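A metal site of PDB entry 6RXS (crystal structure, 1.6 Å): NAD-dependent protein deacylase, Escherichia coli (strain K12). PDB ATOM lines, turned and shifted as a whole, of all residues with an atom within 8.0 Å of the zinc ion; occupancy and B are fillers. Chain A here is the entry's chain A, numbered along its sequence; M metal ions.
Residues that only touch the zinc ion: Ser 133 (3.7 Å). Of the 19 residues printed, 5 come within 4 Å of the zinc ion. The nearest printed residue that does not touch the zinc ion is Ala 156 (4.6 Å).
SG of Cys 130 lies close to N of Ser 133 (3.4 Å). SG of Cys 130 sits close to N of Gln 132. The backbone NH (N) of Cys 130 sits at hydrogen-bond distance from the backbone carbonyl oxygen (O) of Gln 135 (2.9 Å). The side-chain sulfur (SG) of Cys 151 sits close to the side-chain hydroxyl (OG) of Ser 133 (3.2 Å). The backbone NH (N) of Cys 149 lies within hydrogen-bond range of the backbone carbonyl oxygen (O) of Ala 156 (2.9 Å). The backbone NH (N) of Gln 135 lies within hydrogen-bond range of the side-chain hydroxyl (OG) of Ser 133 (2.9 Å).
The zinc ion is bound by SG of Cys 152, SG of Cys 130, SG of Cys 151 and SG of Cys 149. The zinc ion has four donor atoms within binding distance.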
ATOM      1  N   ARG A 129      17.574   2.045  -0.796  1.00  0.00           N
ATOM      2  CA  ARG A 129      17.687   3.426  -0.387  1.00  0.00           C
ATOM      3  C   ARG A 129      17.873   4.291  -1.614  1.00  0.00           C
ATOM      4  O   ARG A 129      18.625   3.949  -2.507  1.00  0.00           O
ATOM      5  CB  ARG A 129      18.848   3.575   0.597  1.00  0.00           C
ATOM      6  CG  ARG A 129      18.894   4.886   1.365  1.00  0.00           C
ATOM      7  CD  ARG A 129      20.134   4.885   2.297  1.00  0.00           C
ATOM      8  NE  ARG A 129      20.015   4.027   3.475  1.00  0.00           N
ATOM      9  CZ  ARG A 129      19.506   4.419   4.644  1.00  0.00           C
ATOM     10  NH1 ARG A 129      19.439   3.573   5.679  1.00  0.00           N
ATOM     11  NH2 ARG A 129      19.065   5.657   4.778  1.00  0.00           N
ATOM     12  N   CYS A 130      17.171   5.421  -1.643  1.00  0.00           N
ATOM     13  CA  CYS A 130      17.384   6.412  -2.699  1.00  0.00           C
ATOM     14  C   CYS A 130      18.789   6.983  -2.578  1.00  0.00           C
ATOM     15  O   CYS A 130      19.176   7.432  -1.492  1.00  0.00           O
ATOM     16  CB  CYS A 130      16.341   7.510  -2.625  1.00  0.00           C
ATOM     17  SG  CYS A 130      16.666   8.791  -3.842  1.00  0.00           S
ATOM     18  N   SER A 131      19.577   6.932  -3.657  1.00  0.00           N
ATOM     19  CA  SER A 131      20.956   7.451  -3.633  1.00  0.00           C
ATOM     20  C   SER A 131      21.013   8.949  -3.371  1.00  0.00           C
ATOM     21  O   SER A 131      22.043   9.482  -2.915  1.00  0.00           O
ATOM     22  CB  SER A 131      21.664   7.163  -4.959  1.00  0.00           C
ATOM     23  OG  SER A 131      21.316   5.900  -5.474  1.00  0.00           O
ATOM     24  N   GLN A 132      19.924   9.647  -3.671  1.00  0.00           N
ATOM     25  CA  GLN A 132      19.907  11.108  -3.504  1.00  0.00           C
ATOM     26  C   GLN A 132      19.324  11.507  -2.146  1.00  0.00           C
ATOM     27  O   GLN A 132      19.978  12.219  -1.374  1.00  0.00           O
ATOM     28  CB  GLN A 132      19.122  11.771  -4.615  1.00  0.00           C
ATOM     29  CG  GLN A 132      18.993  13.260  -4.444  1.00  0.00           C
ATOM     30  CD  GLN A 132      18.251  13.869  -5.615  1.00  0.00           C
ATOM     31  OE1 GLN A 132      18.203  13.277  -6.683  1.00  0.00           O
ATOM     32  NE2 GLN A 132      17.660  15.032  -5.408  1.00  0.00           N
ATOM     33  N   SER A 133      18.104  11.085  -1.854  1.00  0.00           N
ATOM     34  CA  SER A 133      17.427  11.551  -0.639  1.00  0.00           C
ATOM     35  C   SER A 133      17.805  10.773   0.620  1.00  0.00           C
ATOM     36  O   SER A 133      17.626  11.274   1.734  1.00  0.00           O
ATOM     37  CB  SER A 133      15.913  11.459  -0.824  1.00  0.00           C
ATOM     38  OG  SER A 133      15.495  10.112  -0.685  1.00  0.00           O
ATOM     39  N   GLY A 134      18.277   9.538   0.439  1.00  0.00           N
ATOM     40  CA  GLY A 134      18.572   8.653   1.550  1.00  0.00           C
ATOM     41  C   GLY A 134      17.316   7.996   2.099  1.00  0.00           C
ATOM     42  O   GLY A 134      17.373   7.288   3.082  1.00  0.00           O
ATOM     43  N   GLN A 135      16.180   8.232   1.474  1.00  0.00           N
ATOM     44  CA  GLN A 135      14.940   7.652   1.945  1.00  0.00           C
ATOM     45  C   GLN A 135      14.945   6.149   1.699  1.00  0.00           C
ATOM     46  O   GLN A 135      15.483   5.685   0.698  1.00  0.00           O
ATOM     47  CB  GLN A 135      13.734   8.299   1.259  1.00  0.00           C
ATOM     48  CG  GLN A 135      13.498   9.683   1.820  1.00  0.00           C
ATOM     49  CD  GLN A 135      12.247  10.331   1.316  1.00  0.00           C
ATOM     50  OE1 GLN A 135      11.299   9.651   0.887  1.00  0.00           O
ATOM     51  NE2 GLN A 135      12.213  11.648   1.368  1.00  0.00           N
ATOM     52  N   LEU A 137      13.047   2.571   1.076  1.00  0.00           N
ATOM     53  CA  LEU A 137      11.837   2.057   0.434  1.00  0.00           C
ATOM     54  C   LEU A 137      11.787   0.549   0.533  1.00  0.00           C
ATOM     55  O   LEU A 137      12.785  -0.110   0.350  1.00  0.00           O
ATOM     56  CB  LEU A 137      11.775   2.355  -1.065  1.00  0.00           C
ATOM     57  CG  LEU A 137      12.002   3.693  -1.731  1.00  0.00           C
ATOM     58  CD1 LEU A 137      13.401   4.210  -1.430  1.00  0.00           C
ATOM     59  CD2 LEU A 137      11.811   3.393  -3.229  1.00  0.00           C
ATOM     60  N   LYS A 148      14.464   3.197 -10.347  1.00  0.00           N
ATOM     61  CA  LYS A 148      14.652   4.540  -9.789  1.00  0.00           C
ATOM     62  C   LYS A 148      13.696   4.807  -8.628  1.00  0.00           C
ATOM     63  O   LYS A 148      12.703   4.080  -8.436  1.00  0.00           O
ATOM     64  CB  LYS A 148      14.459   5.603 -10.871  1.00  0.00           C
ATOM     65  CG  LYS A 148      15.282   5.416 -12.115  1.00  0.00           C
ATOM     66  CD  LYS A 148      16.745   5.662 -11.867  1.00  0.00           C
ATOM     67  CE  LYS A 148      17.555   5.191 -13.054  1.00  0.00           C
ATOM     68  NZ  LYS A 148      18.212   6.308 -13.782  1.00  0.00           N
ATOM     69  N   CYS A 149      13.988   5.859  -7.860  1.00  0.00           N
ATOM     70  CA  CYS A 149      13.270   6.219  -6.654  1.00  0.00           C
ATOM     71  C   CYS A 149      11.923   6.822  -7.020  1.00  0.00           C
ATOM     72  O   CYS A 149      11.689   7.158  -8.188  1.00  0.00           O
ATOM     73  CB  CYS A 149      14.088   7.208  -5.839  1.00  0.00           C
ATOM     74  SG  CYS A 149      13.865   8.952  -6.375  1.00  0.00           S
ATOM     75  N   HIS A 150      11.041   6.987  -6.030  1.00  0.00           N
ATOM     76  CA  HIS A 150       9.865   7.825  -6.283  1.00  0.00           C
ATOM     77  C   HIS A 150       9.704   8.853  -5.154  1.00  0.00           C
ATOM     78  O   HIS A 150       8.600   9.247  -4.779  1.00  0.00           O
ATOM     79  CB  HIS A 150       8.623   6.957  -6.487  1.00  0.00           C
ATOM     80  CG  HIS A 150       8.429   5.897  -5.449  1.00  0.00           C
ATOM     81  ND1 HIS A 150       9.003   4.655  -5.554  1.00  0.00           N
ATOM     82  CD2 HIS A 150       7.705   5.880  -4.307  1.00  0.00           C
ATOM     83  CE1 HIS A 150       8.644   3.919  -4.518  1.00  0.00           C
ATOM     84  NE2 HIS A 150       7.851   4.636  -3.744  1.00  0.00           N
ATOM     85  N   CYS A 151      10.840   9.322  -4.649  1.00  0.00           N
ATOM     86  CA  CYS A 151      10.837  10.321  -3.604  1.00  0.00           C
ATOM     87  C   CYS A 151      11.394  11.640  -4.103  1.00  0.00           C
ATOM     88  O   CYS A 151      11.215  12.650  -3.446  1.00  0.00           O
ATOM     89  CB  CYS A 151      11.627   9.859  -2.365  1.00  0.00           C
ATOM     90  SG  CYS A 151      13.226   9.073  -2.660  1.00  0.00           S
ATOM     91  N   CYS A 152      12.054  11.633  -5.256  1.00  0.00           N
ATOM     92  CA  CYS A 152      12.744  12.842  -5.725  1.00  0.00           C
ATOM     93  C   CYS A 152      12.072  13.488  -6.950  1.00  0.00           C
ATOM     94  O   CYS A 152      11.365  12.844  -7.726  1.00  0.00           O
ATOM     95  CB  CYS A 152      14.232  12.540  -6.018  1.00  0.00           C
ATOM     96  SG  CYS A 152      15.184  12.055  -4.545  1.00  0.00           S
ATOM     97  N   GLN A 153      12.346  14.782  -7.120  1.00  0.00           N
ATOM     98  CA  GLN A 153      11.752  15.522  -8.235  1.00  0.00           C
ATOM     99  C   GLN A 153      12.032  14.858  -9.565  1.00  0.00           C
ATOM    100  O   GLN A 153      11.184  14.803 -10.446  1.00  0.00           O
ATOM    101  CB  GLN A 153      12.268  16.961  -8.252  1.00  0.00           C
ATOM    102  CG  GLN A 153      11.562  17.818  -9.263  1.00  0.00           C
ATOM    103  CD  GLN A 153      11.995  19.262  -9.182  1.00  0.00           C
ATOM    104  OE1 GLN A 153      12.763  19.624  -8.291  1.00  0.00           O
ATOM    105  NE2 GLN A 153      11.478  20.090 -10.069  1.00  0.00           N
ATOM    106  N   PHE A 154      13.251  14.363  -9.710  1.00  0.00           N
ATOM    107  CA  PHE A 154      13.621  13.570 -10.863  1.00  0.00           C
ATOM    108  C   PHE A 154      14.192  12.261 -10.346  1.00  0.00           C
ATOM    109  O   PHE A 154      15.089  12.266  -9.505  1.00  0.00           O
ATOM    110  CB  PHE A 154      14.598  14.343 -11.759  1.00  0.00           C
ATOM    111  CG  PHE A 154      14.074  15.692 -12.182  1.00  0.00           C
ATOM    112  CD1 PHE A 154      13.173  15.796 -13.222  1.00  0.00           C
ATOM    113  CD2 PHE A 154      14.427  16.831 -11.495  1.00  0.00           C
ATOM    114  CE1 PHE A 154      12.629  17.003 -13.567  1.00  0.00           C
ATOM    115  CE2 PHE A 154      13.899  18.063 -11.853  1.00  0.00           C
ATOM    116  CZ  PHE A 154      13.011  18.144 -12.903  1.00  0.00           C
ATOM    117  N   PRO A 155      13.584  11.141 -10.751  1.00  0.00           N
ATOM    118  CA  PRO A 155      13.957   9.899 -10.046  1.00  0.00           C
ATOM    119  C   PRO A 155      15.453   9.600 -10.112  1.00  0.00           C
ATOM    120  O   PRO A 155      16.072   9.724 -11.155  1.00  0.00           O
ATOM    121  CB  PRO A 155      13.136   8.832 -10.783  1.00  0.00           C
ATOM    122  CG  PRO A 155      11.915   9.559 -11.228  1.00  0.00           C
ATOM    123  CD  PRO A 155      12.369  10.959 -11.569  1.00  0.00           C
ATOM    124  N   ALA A 156      16.012   9.229  -8.952  1.00  0.00           N
ATOM    125  CA  ALA A 156      17.439   8.939  -8.783  1.00  0.00           C
ATOM    126  C   ALA A 156      17.687   7.427  -8.698  1.00  0.00           C
ATOM    127  O   ALA A 156      16.765   6.689  -8.383  1.00  0.00           O
ATOM    128  CB  ALA A 156      17.929   9.588  -7.555  1.00  0.00           C
ATOM    129  N   PRO A 157      18.942   6.989  -8.908  1.00  0.00           N
ATOM    130  CA  PRO A 157      19.247   5.552  -8.738  1.00  0.00           C
ATOM    131  C   PRO A 157      18.981   5.054  -7.318  1.00  0.00           C
ATOM    132  O   PRO A 157      19.030   5.881  -6.370  1.00  0.00           O
ATOM    133  CB  PRO A 157      20.735   5.467  -9.050  1.00  0.00           C
ATOM    134  CG  PRO A 157      21.048   6.704  -9.852  1.00  0.00           C
ATOM    135  CD  PRO A 157      20.108   7.763  -9.365  1.00  0.00           C
ATOM    136  N   LEU A 158      18.724   3.760  -7.204  1.00  0.00           N
ATOM    137  CA  LEU A 158      18.518   3.066  -5.936  1.00  0.00           C
ATOM    138  C   LEU A 158      19.807   2.378  -5.512  1.00  0.00           C
ATOM    139  O   LEU A 158      20.577   1.913  -6.360  1.00  0.00           O
ATOM    140  CB  LEU A 158      17.398   2.039  -6.071  1.00  0.00           C
ATOM    141  CG  LEU A 158      16.055   2.650  -6.510  1.00  0.00           C
ATOM    142  CD1 LEU A 158      15.019   1.582  -6.804  1.00  0.00           C
ATOM    143  CD2 LEU A 158      15.561   3.629  -5.452  1.00  0.00           C
HETATM  144 ZN    ZN M   1      14.696   9.884  -4.323  1.00  0.00          ZN
